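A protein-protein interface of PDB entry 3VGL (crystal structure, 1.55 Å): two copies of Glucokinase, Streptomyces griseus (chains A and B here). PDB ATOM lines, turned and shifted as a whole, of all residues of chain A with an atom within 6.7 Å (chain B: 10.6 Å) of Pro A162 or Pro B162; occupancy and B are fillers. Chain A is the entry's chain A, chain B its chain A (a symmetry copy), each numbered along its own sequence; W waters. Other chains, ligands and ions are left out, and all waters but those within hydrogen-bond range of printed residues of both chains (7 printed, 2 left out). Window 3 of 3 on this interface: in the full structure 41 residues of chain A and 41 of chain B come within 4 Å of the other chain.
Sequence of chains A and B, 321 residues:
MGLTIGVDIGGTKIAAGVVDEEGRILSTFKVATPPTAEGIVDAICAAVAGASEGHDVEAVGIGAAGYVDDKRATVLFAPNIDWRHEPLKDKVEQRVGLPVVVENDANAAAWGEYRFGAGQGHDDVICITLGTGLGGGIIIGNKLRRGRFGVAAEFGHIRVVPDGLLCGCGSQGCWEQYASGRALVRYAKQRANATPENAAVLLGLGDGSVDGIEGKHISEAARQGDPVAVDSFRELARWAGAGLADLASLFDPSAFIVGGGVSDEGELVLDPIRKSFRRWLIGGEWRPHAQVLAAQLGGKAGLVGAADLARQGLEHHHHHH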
ATOM      1  N   ARG A 159       7.649  18.249  15.897  1.00  0.00           N
ATOM      2  CA  ARG A 159       6.725  19.350  15.578  1.00  0.00           C
ATOM      3  C   ARG A 159       6.628  19.495  14.074  1.00  0.00           C
ATOM      4  O   ARG A 159       7.622  19.830  13.396  1.00  0.00           O
ATOM      5  CB  ARG A 159       7.241  20.652  16.175  1.00  0.00           C
ATOM      6  CG  ARG A 159       6.281  21.795  15.929  1.00  0.00           C
ATOM      7  CD  ARG A 159       6.805  23.124  16.446  1.00  0.00           C
ATOM      8  NE  ARG A 159       7.924  23.625  15.645  1.00  0.00           N
ATOM      9  CZ  ARG A 159       8.466  24.823  15.808  1.00  0.00           C
ATOM     10  NH1 ARG A 159       9.511  25.191  15.066  1.00  0.00           N
ATOM     11  NH2 ARG A 159       7.941  25.666  16.696  1.00  0.00           N
ATOM     12  N   VAL A 160       5.455  19.214  13.552  1.00  0.00           N
ATOM     13  CA  VAL A 160       5.225  19.337  12.114  1.00  0.00           C
ATOM     14  C   VAL A 160       4.517  20.636  11.746  1.00  0.00           C
ATOM     15  O   VAL A 160       4.694  21.103  10.613  1.00  0.00           O
ATOM     16  CB  VAL A 160       4.507  18.105  11.496  1.00  0.00           C
ATOM     17  CG1 VAL A 160       5.368  16.852  11.700  1.00  0.00           C
ATOM     18  CG2 VAL A 160       3.106  17.900  12.046  1.00  0.00           C
ATOM     19  N   VAL A 161       3.739  21.223  12.669  1.00  0.00           N
ATOM     20  CA  VAL A 161       3.074  22.512  12.394  1.00  0.00           C
ATOM     21  C   VAL A 161       3.448  23.454  13.522  1.00  0.00           C
ATOM     22  O   VAL A 161       3.003  23.258  14.650  1.00  0.00           O
ATOM     23  CB  VAL A 161       1.530  22.399  12.325  1.00  0.00           C
ATOM     24  CG1 VAL A 161       0.899  23.791  12.182  1.00  0.00           C
ATOM     25  CG2 VAL A 161       1.129  21.516  11.146  1.00  0.00           C
ATOM     26  N   PRO A 162       4.297  24.456  13.253  1.00  0.00           N
ATOM     27  CA  PRO A 162       4.599  25.394  14.343  1.00  0.00           C
ATOM     28  C   PRO A 162       3.302  26.025  14.877  1.00  0.00           C
ATOM     29  O   PRO A 162       2.444  26.444  14.091  1.00  0.00           O
ATOM     30  CB  PRO A 162       5.462  26.459  13.661  1.00  0.00           C
ATOM     31  CG  PRO A 162       6.138  25.687  12.523  1.00  0.00           C
ATOM     32  CD  PRO A 162       5.017  24.788  12.001  1.00  0.00           C
ATOM     33  N   ASP A 163       3.190  26.088  16.204  1.00  0.00           N
ATOM     34  CA  ASP A 163       1.996  26.664  16.835  1.00  0.00           C
ATOM     35  C   ASP A 163       0.722  25.925  16.428  1.00  0.00           C
ATOM     36  O   ASP A 163      -0.351  26.517  16.456  1.00  0.00           O
ATOM     37  CB  ASP A 163       1.903  28.189  16.594  1.00  0.00           C
ATOM     38  CG  ASP A 163       3.156  28.907  17.044  1.00  0.00           C
ATOM     39  OD1 ASP A 163       3.386  28.964  18.272  1.00  0.00           O
ATOM     40  OD2 ASP A 163       3.907  29.397  16.158  1.00  0.00           O
ATOM     41  N   GLY A 164       0.850  24.634  16.108  1.00  0.00           N
ATOM     42  CA  GLY A 164      -0.297  23.803  15.675  1.00  0.00           C
ATOM     43  C   GLY A 164      -1.136  23.204  16.793  1.00  0.00           C
ATOM     44  O   GLY A 164      -1.220  23.730  17.890  1.00  0.00           O
ATOM     45  N   LEU A 165      -1.772  22.081  16.483  1.00  0.00           N
ATOM     46  CA  LEU A 165      -2.750  21.473  17.394  1.00  0.00           C
ATOM     47  C   LEU A 165      -2.169  21.121  18.763  1.00  0.00           C
ATOM     48  O   LEU A 165      -1.059  20.620  18.846  1.00  0.00           O
ATOM     49  CB  LEU A 165      -3.239  20.172  16.749  1.00  0.00           C
ATOM     50  CG  LEU A 165      -4.230  20.365  15.603  1.00  0.00           C
ATOM     51  CD1 LEU A 165      -4.371  19.030  14.840  1.00  0.00           C
ATOM     52  CD2 LEU A 165      -5.609  20.870  16.131  1.00  0.00           C
ATOM     53  N   GLN A 172       2.569  21.794  21.146  1.00  0.00           N
ATOM     54  CA  GLN A 172       1.683  22.042  20.002  1.00  0.00           C
ATOM     55  C   GLN A 172       2.317  21.577  18.711  1.00  0.00           C
ATOM     56  O   GLN A 172       3.530  21.709  18.508  1.00  0.00           O
ATOM     57  CB  GLN A 172       1.447  23.552  19.856  1.00  0.00           C
ATOM     58  CG  GLN A 172       0.419  24.108  20.817  1.00  0.00           C
ATOM     59  CD  GLN A 172       0.278  25.601  20.672  1.00  0.00           C
ATOM     60  OE1 GLN A 172      -0.247  26.109  19.652  1.00  0.00           O
ATOM     61  NE2 GLN A 172       0.754  26.332  21.670  1.00  0.00           N
ATOM     62  N   GLY A 173       1.468  21.104  17.809  1.00  0.00           N
ATOM     63  CA  GLY A 173       1.893  20.830  16.426  1.00  0.00           C
ATOM     64  C   GLY A 173       2.557  19.492  16.195  1.00  0.00           C
ATOM     65  O   GLY A 173       3.108  19.246  15.119  1.00  0.00           O
ATOM     66  N   TYR A 178      -1.657  14.912  13.709  1.00  0.00           N
ATOM     67  CA  TYR A 178      -1.972  14.947  12.264  1.00  0.00           C
ATOM     68  C   TYR A 178      -1.970  13.569  11.635  1.00  0.00           C
ATOM     69  O   TYR A 178      -2.638  13.351  10.620  1.00  0.00           O
ATOM     70  CB  TYR A 178      -0.987  15.866  11.519  1.00  0.00           C
ATOM     71  CG  TYR A 178      -1.035  17.275  12.073  1.00  0.00           C
ATOM     72  CD1 TYR A 178      -1.992  18.177  11.625  1.00  0.00           C
ATOM     73  CD2 TYR A 178      -0.200  17.649  13.130  1.00  0.00           C
ATOM     74  CE1 TYR A 178      -2.077  19.470  12.162  1.00  0.00           C
ATOM     75  CE2 TYR A 178      -0.269  18.937  13.672  1.00  0.00           C
ATOM     76  CZ  TYR A 178      -1.219  19.819  13.185  1.00  0.00           C
ATOM     77  OH  TYR A 178      -1.355  21.107  13.697  1.00  0.00           O
ATOM     78  N   ARG A 238      -1.481  12.324   3.667  1.00  0.00           N
ATOM     79  CA  ARG A 238      -0.767  13.584   3.461  1.00  0.00           C
ATOM     80  C   ARG A 238       0.250  13.784   4.572  1.00  0.00           C
ATOM     81  O   ARG A 238       1.441  14.038   4.333  1.00  0.00           O
ATOM     82  CB  ARG A 238      -1.788  14.745   3.436  1.00  0.00           C
ATOM     83  CG  ARG A 238      -1.213  16.175   3.559  1.00  0.00           C
ATOM     84  CD  ARG A 238      -2.374  17.174   3.843  1.00  0.00           C
ATOM     85  NE  ARG A 238      -1.919  18.544   4.081  1.00  0.00           N
ATOM     86  CZ  ARG A 238      -2.673  19.538   4.558  1.00  0.00           C
ATOM     87  NH1 ARG A 238      -3.955  19.350   4.862  1.00  0.00           N
ATOM     88  NH2 ARG A 238      -2.138  20.743   4.729  1.00  0.00           N
ATOM     89  N   TRP A 239      -0.225  13.642   5.799  1.00  0.00           N
ATOM     90  CA  TRP A 239       0.647  13.889   6.942  1.00  0.00           C
ATOM     91  C   TRP A 239       1.550  12.700   7.243  1.00  0.00           C
ATOM     92  O   TRP A 239       2.724  12.894   7.650  1.00  0.00           O
ATOM     93  CB  TRP A 239      -0.192  14.233   8.163  1.00  0.00           C
ATOM     94  CG  TRP A 239      -0.917  15.515   7.992  1.00  0.00           C
ATOM     95  CD1 TRP A 239      -2.249  15.675   7.685  1.00  0.00           C
ATOM     96  CD2 TRP A 239      -0.378  16.827   8.150  1.00  0.00           C
ATOM     97  NE1 TRP A 239      -2.553  17.021   7.619  1.00  0.00           N
ATOM     98  CE2 TRP A 239      -1.423  17.743   7.895  1.00  0.00           C
ATOM     99  CE3 TRP A 239       0.893  17.313   8.463  1.00  0.00           C
ATOM    100  CZ2 TRP A 239      -1.231  19.145   7.973  1.00  0.00           C
ATOM    101  CZ3 TRP A 239       1.090  18.724   8.527  1.00  0.00           C
ATOM    102  CH2 TRP A 239       0.022  19.599   8.286  1.00  0.00           C
ATOM    103  N   HIS B 157      16.891  19.271   5.403  1.00  0.00           N
ATOM    104  CA  HIS B 157      15.711  19.204   4.538  1.00  0.00           C
ATOM    105  C   HIS B 157      14.514  18.533   5.180  1.00  0.00           C
ATOM    106  O   HIS B 157      13.543  18.185   4.513  1.00  0.00           O
ATOM    107  CB  HIS B 157      16.099  18.604   3.167  1.00  0.00           C
ATOM    108  CG  HIS B 157      17.299  19.274   2.610  1.00  0.00           C
ATOM    109  ND1 HIS B 157      17.252  20.557   2.102  1.00  0.00           N
ATOM    110  CD2 HIS B 157      18.610  18.910   2.641  1.00  0.00           C
ATOM    111  CE1 HIS B 157      18.484  20.934   1.790  1.00  0.00           C
ATOM    112  NE2 HIS B 157      19.323  19.959   2.109  1.00  0.00           N
ATOM    113  N   ILE B 158      14.555  18.428   6.505  1.00  0.00           N
ATOM    114  CA  ILE B 158      13.341  18.092   7.268  1.00  0.00           C
ATOM    115  C   ILE B 158      12.416  19.302   7.169  1.00  0.00           C
ATOM    116  O   ILE B 158      12.861  20.443   7.269  1.00  0.00           O
ATOM    117  CB  ILE B 158      13.693  17.871   8.767  1.00  0.00           C
ATOM    118  CG1 ILE B 158      14.554  16.605   8.906  1.00  0.00           C
ATOM    119  CG2 ILE B 158      12.422  17.779   9.637  1.00  0.00           C
ATOM    120  CD1 ILE B 158      15.308  16.621  10.250  1.00  0.00           C
ATOM    121  N   ARG B 159      11.133  19.076   6.961  1.00  0.00           N
ATOM    122  CA  ARG B 159      10.191  20.191   6.758  1.00  0.00           C
ATOM    123  C   ARG B 159       9.735  20.705   8.107  1.00  0.00           C
ATOM    124  O   ARG B 159       9.067  19.982   8.877  1.00  0.00           O
ATOM    125  CB  ARG B 159       8.982  19.714   5.968  1.00  0.00           C
ATOM    126  CG  ARG B 159       8.025  20.850   5.677  1.00  0.00           C
ATOM    127  CD  ARG B 159       6.770  20.390   4.955  1.00  0.00           C
ATOM    128  NE  ARG B 159       5.891  19.603   5.824  1.00  0.00           N
ATOM    129  CZ  ARG B 159       4.678  19.203   5.473  1.00  0.00           C
ATOM    130  NH1 ARG B 159       3.954  18.454   6.305  1.00  0.00           N
ATOM    131  NH2 ARG B 159       4.176  19.580   4.298  1.00  0.00           N
ATOM    132  N   VAL B 160      10.117  21.926   8.408  1.00  0.00           N
ATOM    133  CA  VAL B 160       9.722  22.546   9.671  1.00  0.00           C
ATOM    134  C   VAL B 160       8.539  23.494   9.510  1.00  0.00           C
ATOM    135  O   VAL B 160       7.804  23.690  10.487  1.00  0.00           O
ATOM    136  CB  VAL B 160      10.900  23.230  10.418  1.00  0.00           C
ATOM    137  CG1 VAL B 160      11.972  22.186  10.754  1.00  0.00           C
ATOM    138  CG2 VAL B 160      11.496  24.392   9.643  1.00  0.00           C
ATOM    139  N   VAL B 161       8.339  24.069   8.314  1.00  0.00           N
ATOM    140  CA  VAL B 161       7.179  24.949   8.078  1.00  0.00           C
ATOM    141  C   VAL B 161       6.459  24.418   6.854  1.00  0.00           C
ATOM    142  O   VAL B 161       6.987  24.515   5.749  1.00  0.00           O
ATOM    143  CB  VAL B 161       7.575  26.426   7.826  1.00  0.00           C
ATOM    144  CG1 VAL B 161       6.339  27.254   7.447  1.00  0.00           C
ATOM    145  CG2 VAL B 161       8.232  27.005   9.077  1.00  0.00           C
ATOM    146  N   PRO B 162       5.276  23.814   7.028  1.00  0.00           N
ATOM    147  CA  PRO B 162       4.566  23.361   5.825  1.00  0.00           C
ATOM    148  C   PRO B 162       4.339  24.541   4.864  1.00  0.00           C
ATOM    149  O   PRO B 162       3.932  25.626   5.297  1.00  0.00           O
ATOM    150  CB  PRO B 162       3.226  22.862   6.374  1.00  0.00           C
ATOM    151  CG  PRO B 162       3.574  22.417   7.798  1.00  0.00           C
ATOM    152  CD  PRO B 162       4.535  23.506   8.275  1.00  0.00           C
ATOM    153  N   ASP B 163       4.598  24.302   3.579  1.00  0.00           N
ATOM    154  CA  ASP B 163       4.426  25.350   2.566  1.00  0.00           C
ATOM    155  C   ASP B 163       5.291  26.575   2.858  1.00  0.00           C
ATOM    156  O   ASP B 163       4.944  27.672   2.433  1.00  0.00           O
ATOM    157  CB  ASP B 163       2.935  25.708   2.363  1.00  0.00           C
ATOM    158  CG  ASP B 163       2.104  24.489   2.032  1.00  0.00           C
ATOM    159  OD1 ASP B 163       2.280  23.949   0.917  1.00  0.00           O
ATOM    160  OD2 ASP B 163       1.290  24.074   2.900  1.00  0.00           O
ATOM    161  N   GLY B 164       6.426  26.365   3.532  1.00  0.00           N
ATOM    162  CA  GLY B 164       7.348  27.465   3.902  1.00  0.00           C
ATOM    163  C   GLY B 164       8.336  27.887   2.825  1.00  0.00           C
ATOM    164  O   GLY B 164       8.097  27.744   1.638  1.00  0.00           O
ATOM    165  N   LEU B 165       9.463  28.425   3.272  1.00  0.00           N
ATOM    166  CA  LEU B 165      10.441  29.034   2.362  1.00  0.00           C
ATOM    167  C   LEU B 165      10.970  28.067   1.303  1.00  0.00           C
ATOM    168  O   LEU B 165      11.248  26.918   1.609  1.00  0.00           O
ATOM    169  CB  LEU B 165      11.634  29.497   3.204  1.00  0.00           C
ATOM    170  CG  LEU B 165      11.388  30.775   4.003  1.00  0.00           C
ATOM    171  CD1 LEU B 165      12.518  30.934   5.043  1.00  0.00           C
ATOM    172  CD2 LEU B 165      11.297  32.018   3.064  1.00  0.00           C
ATOM    173  N   LEU B 166      11.160  28.555   0.075  1.00  0.00           N
ATOM    174  CA  LEU B 166      11.827  27.762  -0.961  1.00  0.00           C
ATOM    175  C   LEU B 166      13.247  27.396  -0.570  1.00  0.00           C
ATOM    176  O   LEU B 166      14.009  28.264  -0.123  1.00  0.00           O
ATOM    177  CB  LEU B 166      11.847  28.545  -2.277  1.00  0.00           C
ATOM    178  CG  LEU B 166      10.515  28.889  -2.925  1.00  0.00           C
ATOM    179  CD1 LEU B 166      10.782  29.901  -4.029  1.00  0.00           C
ATOM    180  CD2 LEU B 166       9.842  27.650  -3.480  1.00  0.00           C
ATOM    181  N   SER B 171      12.364  21.782  -2.538  1.00  0.00           N
ATOM    182  CA  SER B 171      11.175  21.693  -1.659  1.00  0.00           C
ATOM    183  C   SER B 171      10.965  22.977  -0.881  1.00  0.00           C
ATOM    184  O   SER B 171      11.734  23.936  -1.038  1.00  0.00           O
ATOM    185  CB  SER B 171      11.383  20.553  -0.665  1.00  0.00           C
ATOM    186  OG  SER B 171      11.294  19.308  -1.378  1.00  0.00           O
ATOM    187  N   GLN B 172       9.929  22.999  -0.045  1.00  0.00           N
ATOM    188  CA  GLN B 172       9.610  24.183   0.761  1.00  0.00           C
ATOM    189  C   GLN B 172       9.639  23.860   2.238  1.00  0.00           C
ATOM    190  O   GLN B 172       9.228  22.775   2.665  1.00  0.00           O
ATOM    191  CB  GLN B 172       8.183  24.650   0.442  1.00  0.00           C
ATOM    192  CG  GLN B 172       8.070  25.450  -0.838  1.00  0.00           C
ATOM    193  CD  GLN B 172       6.641  25.823  -1.133  1.00  0.00           C
ATOM    194  OE1 GLN B 172       6.031  26.665  -0.430  1.00  0.00           O
ATOM    195  NE2 GLN B 172       6.074  25.200  -2.156  1.00  0.00           N
ATOM    196  N   GLY B 173      10.055  24.848   3.018  1.00  0.00           N
ATOM    197  CA  GLY B 173       9.922  24.774   4.484  1.00  0.00           C
ATOM    198  C   GLY B 173      11.017  24.023   5.206  1.00  0.00           C
ATOM    199  O   GLY B 173      10.901  23.751   6.404  1.00  0.00           O
ATOM    200  N   CYS B 174      12.064  23.672   4.481  1.00  0.00           N
ATOM    201  CA  CYS B 174      13.209  22.952   5.056  1.00  0.00           C
ATOM    202  C   CYS B 174      13.873  23.671   6.224  1.00  0.00           C
ATOM    203  O   CYS B 174      14.051  24.917   6.235  1.00  0.00           O
ATOM    204  CB  CYS B 174      14.236  22.761   3.963  1.00  0.00           C
ATOM    205  SG  CYS B 174      13.675  21.770   2.594  1.00  0.00           S
ATOM    206  N   TRP B 175      14.270  22.875   7.223  1.00  0.00           N
ATOM    207  CA  TRP B 175      14.950  23.419   8.390  1.00  0.00           C
ATOM    208  C   TRP B 175      16.102  24.379   8.029  1.00  0.00           C
ATOM    209  O   TRP B 175      16.265  25.423   8.650  1.00  0.00           O
ATOM    210  CB  TRP B 175      15.435  22.260   9.284  1.00  0.00           C
ATOM    211  CG  TRP B 175      15.915  22.674  10.657  1.00  0.00           C
ATOM    212  CD1 TRP B 175      15.609  23.831  11.351  1.00  0.00           C
ATOM    213  CD2 TRP B 175      16.690  21.869  11.531  1.00  0.00           C
ATOM    214  NE1 TRP B 175      16.217  23.802  12.590  1.00  0.00           N
ATOM    215  CE2 TRP B 175      16.869  22.600  12.728  1.00  0.00           C
ATOM    216  CE3 TRP B 175      17.262  20.593  11.411  1.00  0.00           C
ATOM    217  CZ2 TRP B 175      17.623  22.104  13.807  1.00  0.00           C
ATOM    218  CZ3 TRP B 175      17.995  20.086  12.491  1.00  0.00           C
ATOM    219  CH2 TRP B 175      18.175  20.853  13.667  1.00  0.00           C
ATOM    220  N   TYR B 178      15.659  28.094   7.812  1.00  0.00           N
ATOM    221  CA  TYR B 178      15.364  28.784   9.086  1.00  0.00           C
ATOM    222  C   TYR B 178      16.537  28.766  10.044  1.00  0.00           C
ATOM    223  O   TYR B 178      16.648  29.644  10.903  1.00  0.00           O
ATOM    224  CB  TYR B 178      14.125  28.167   9.760  1.00  0.00           C
ATOM    225  CG  TYR B 178      12.914  28.254   8.854  1.00  0.00           C
ATOM    226  CD1 TYR B 178      12.142  29.408   8.818  1.00  0.00           C
ATOM    227  CD2 TYR B 178      12.630  27.225   7.951  1.00  0.00           C
ATOM    228  CE1 TYR B 178      11.045  29.519   7.951  1.00  0.00           C
ATOM    229  CE2 TYR B 178      11.536  27.319   7.084  1.00  0.00           C
ATOM    230  CZ  TYR B 178      10.773  28.474   7.091  1.00  0.00           C
ATOM    231  OH  TYR B 178       9.685  28.640   6.237  1.00  0.00           O
ATOM    232  N   GLU B 235      16.620  34.801  16.820  1.00  0.00           N
ATOM    233  CA  GLU B 235      15.758  34.171  15.818  1.00  0.00           C
ATOM    234  C   GLU B 235      16.398  32.881  15.300  1.00  0.00           C
ATOM    235  O   GLU B 235      15.707  31.864  15.142  1.00  0.00           O
ATOM    236  CB  GLU B 235      15.437  35.152  14.661  1.00  0.00           C
ATOM    237  CG  GLU B 235      14.496  34.611  13.588  1.00  0.00           C
ATOM    238  CD  GLU B 235      13.059  34.467  14.024  1.00  0.00           C
ATOM    239  OE1 GLU B 235      12.685  35.003  15.087  1.00  0.00           O
ATOM    240  OE2 GLU B 235      12.287  33.801  13.296  1.00  0.00           O
ATOM    241  N   ARG B 238      15.839  30.259  17.953  1.00  0.00           N
ATOM    242  CA  ARG B 238      14.449  29.801  17.970  1.00  0.00           C
ATOM    243  C   ARG B 238      14.308  28.561  17.105  1.00  0.00           C
ATOM    244  O   ARG B 238      13.778  27.523  17.528  1.00  0.00           O
ATOM    245  CB  ARG B 238      13.537  30.939  17.455  1.00  0.00           C
ATOM    246  CG  ARG B 238      12.087  30.549  17.087  1.00  0.00           C
ATOM    247  CD  ARG B 238      11.426  31.715  16.294  1.00  0.00           C
ATOM    248  NE  ARG B 238      10.082  31.401  15.807  1.00  0.00           N
ATOM    249  CZ  ARG B 238       9.389  32.127  14.925  1.00  0.00           C
ATOM    250  NH1 ARG B 238       9.890  33.244  14.403  1.00  0.00           N
ATOM    251  NH2 ARG B 238       8.173  31.733  14.563  1.00  0.00           N
ATOM    252  N   TRP B 239      14.812  28.668  15.886  1.00  0.00           N
ATOM    253  CA  TRP B 239      14.661  27.564  14.944  1.00  0.00           C
ATOM    254  C   TRP B 239      15.686  26.462  15.183  1.00  0.00           C
ATOM    255  O   TRP B 239      15.361  25.259  15.013  1.00  0.00           O
ATOM    256  CB  TRP B 239      14.773  28.085  13.520  1.00  0.00           C
ATOM    257  CG  TRP B 239      13.654  28.994  13.175  1.00  0.00           C
ATOM    258  CD1 TRP B 239      13.695  30.369  13.121  1.00  0.00           C
ATOM    259  CD2 TRP B 239      12.331  28.614  12.798  1.00  0.00           C
ATOM    260  NE1 TRP B 239      12.455  30.858  12.756  1.00  0.00           N
ATOM    261  CE2 TRP B 239      11.605  29.802  12.558  1.00  0.00           C
ATOM    262  CE3 TRP B 239      11.686  27.382  12.661  1.00  0.00           C
ATOM    263  CZ2 TRP B 239      10.247  29.786  12.154  1.00  0.00           C
ATOM    264  CZ3 TRP B 239      10.316  27.367  12.268  1.00  0.00           C
ATOM    265  CH2 TRP B 239       9.637  28.568  12.020  1.00  0.00           C
ATOM    266  N   ALA B 242      14.547  24.603  18.494  1.00  0.00           N
ATOM    267  CA  ALA B 242      13.330  23.803  18.260  1.00  0.00           C
ATOM    268  C   ALA B 242      13.659  22.548  17.475  1.00  0.00           C
ATOM    269  O   ALA B 242      13.137  21.459  17.770  1.00  0.00           O
ATOM    270  CB  ALA B 242      12.252  24.616  17.534  1.00  0.00           C
ATOM    271  N   GLY B 243      14.528  22.672  16.476  1.00  0.00           N
ATOM    272  CA  GLY B 243      14.930  21.510  15.701  1.00  0.00           C
ATOM    273  C   GLY B 243      15.735  20.524  16.525  1.00  0.00           C
ATOM    274  O   GLY B 243      15.594  19.321  16.352  1.00  0.00           O
ATOM    275  N   ASP B 246      13.387  18.507  18.420  1.00  0.00           N
ATOM    276  CA  ASP B 246      12.871  17.412  17.548  1.00  0.00           C
ATOM    277  C   ASP B 246      13.897  16.267  17.377  1.00  0.00           C
ATOM    278  O   ASP B 246      13.551  15.073  17.394  1.00  0.00           O
ATOM    279  CB  ASP B 246      12.448  17.940  16.171  1.00  0.00           C
ATOM    280  CG  ASP B 246      11.152  18.780  16.215  1.00  0.00           C
ATOM    281  OD1 ASP B 246      10.393  18.716  17.191  1.00  0.00           O
ATOM    282  OD2 ASP B 246      10.940  19.537  15.249  1.00  0.00           O
ATOM    283  N   TRP B 280      12.080  24.072  24.223  1.00  0.00           N
ATOM    284  CA  TRP B 280      11.281  23.254  23.315  1.00  0.00           C
ATOM    285  C   TRP B 280      11.229  21.764  23.642  1.00  0.00           C
ATOM    286  O   TRP B 280      10.347  21.069  23.168  1.00  0.00           O
ATOM    287  CB  TRP B 280      11.771  23.431  21.867  1.00  0.00           C
ATOM    288  CG  TRP B 280      11.526  24.778  21.295  1.00  0.00           C
ATOM    289  CD1 TRP B 280      12.462  25.749  21.049  1.00  0.00           C
ATOM    290  CD2 TRP B 280      10.271  25.309  20.863  1.00  0.00           C
ATOM    291  NE1 TRP B 280      11.859  26.862  20.510  1.00  0.00           N
ATOM    292  CE2 TRP B 280      10.514  26.613  20.379  1.00  0.00           C
ATOM    293  CE3 TRP B 280       8.960  24.816  20.851  1.00  0.00           C
ATOM    294  CZ2 TRP B 280       9.493  27.431  19.876  1.00  0.00           C
ATOM    295  CZ3 TRP B 280       7.954  25.627  20.362  1.00  0.00           C
ATOM    296  CH2 TRP B 280       8.229  26.919  19.878  1.00  0.00           C
HETATM  297  O   HOH W   1       6.669  29.431  14.943  1.00  0.00           O
HETATM  298  O   HOH W   2       6.255  19.864   8.776  1.00  0.00           O
HETATM  299  O   HOH W   3      11.078  22.400  14.380  1.00  0.00           O
HETATM  300  O   HOH W   4      10.756  27.364  16.476  1.00  0.00           O
HETATM  301  O   HOH W   5       8.266  22.524  12.890  1.00  0.00           O
HETATM  302  O   HOH W   6       1.951  17.180   4.683  1.00  0.00           O
HETATM  303  O   HOH W   7       0.440  21.767   4.650  1.00  0.00           O
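The side-chain carboxylate (OD1) of Asp B246 lies within hydrogen-bond range of the backbone NH (N) of Arg A159 (3.1 Å).
Pro A162 touches two residues of chain B. Of chain A, only Val A160 and Pro A162 come within 4 Å of Pro B162. No residue of chain B comes within 4 Å of Val A161. No residue of chain B comes within 4 Å of Asp A163. No residue of chain B comes within 4 Å of Gly A164. Gly A173 touches none of the printed residues of chain B. Of the printed residues of chain A, Val B160 touches Pro A162. Printed residues of chain B within 4 Å of Val A160: Pro B162 (3.3 Å). Of the printed residues of chain B, Trp A239 touches Arg B159. Gln B172 touches none of the printed residues of chain A.
Trp B239 touches Arg A159. NH1 of Arg A159 touches CB of Ala B242, at 3.7 Å. Trp B280 touches Arg A159 (CH2 to NH2, 3.4 Å). CG of Pro B162 touches O of Val A160, at 3.3 Å. CG of Pro A162 touches O of Val B160 (3.3 Å). Pro B162 touches Pro A162 (CD to CD, 3.97 Å). Trp A239 touches Arg B159 (CZ3 to NH1, 3.6 Å).
Arg A159 touches Trp B239, and with the chains exchanged Trp A239 touches Arg B159. Val A160 touches Pro B162, and with the chains exchanged Pro A162 touches Val B160. Pro B162 touches its own counterpart, Pro A162. Of the 8 pairs that touch across the chains among the printed residues, 5 have their exchanged pair printed and touching as well.
Printed residues of chain A that touch a printed residue of chain B: Arg A159, Val A160, Pro A162 and Trp A239. Along chain A the printed residues that touch a printed residue of chain B span positions 159 to 239. Among the printed residues, 8 pairs touch across the chains. Among the printed residues, no Asp or Glu carboxylate lies within 4 Å of a Lys or Arg side-chain nitrogen of the other chain.
The backbone NH (N) of Val A160 is in hydrogen-bond range of the backbone carbonyl oxygen (O) of Gly A173. The backbone carbonyl oxygen of Gly B173 lies within hydrogen-bond range of the backbone NH of Val B160, at 2.8 Å. The indole nitrogen (NE1) of Trp B175 lies within hydrogen-bond range of the backbone carbonyl oxygen (O) of Trp B239 (3.0 Å). The indole nitrogen (NE1) of Trp B239 is in hydrogen-bond range of the side-chain carboxylate (OE2) of Glu B235.
Water W2 lies within hydrogen-bond range of the backbone carbonyl oxygen of Val A160 (2.7 Å) and the backbone carbonyl oxygen of Arg B159 (2.8 Å). Water W5 bridges the backbone carbonyl oxygen of Val B160 (2.7 Å) and the backbone carbonyl oxygen of Arg A159 (2.8 Å). Water W1 bridges the guanidinium group of Arg B238 (2.8 Å) and the side-chain carboxylate of Asp A163 (3.0 Å). Water W3 lies within hydrogen-bond range of the side-chain carboxylate (OD2) of Asp B246 (3.0 Å) and the guanidinium group (NH1) of Arg A159 (3.3 Å).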
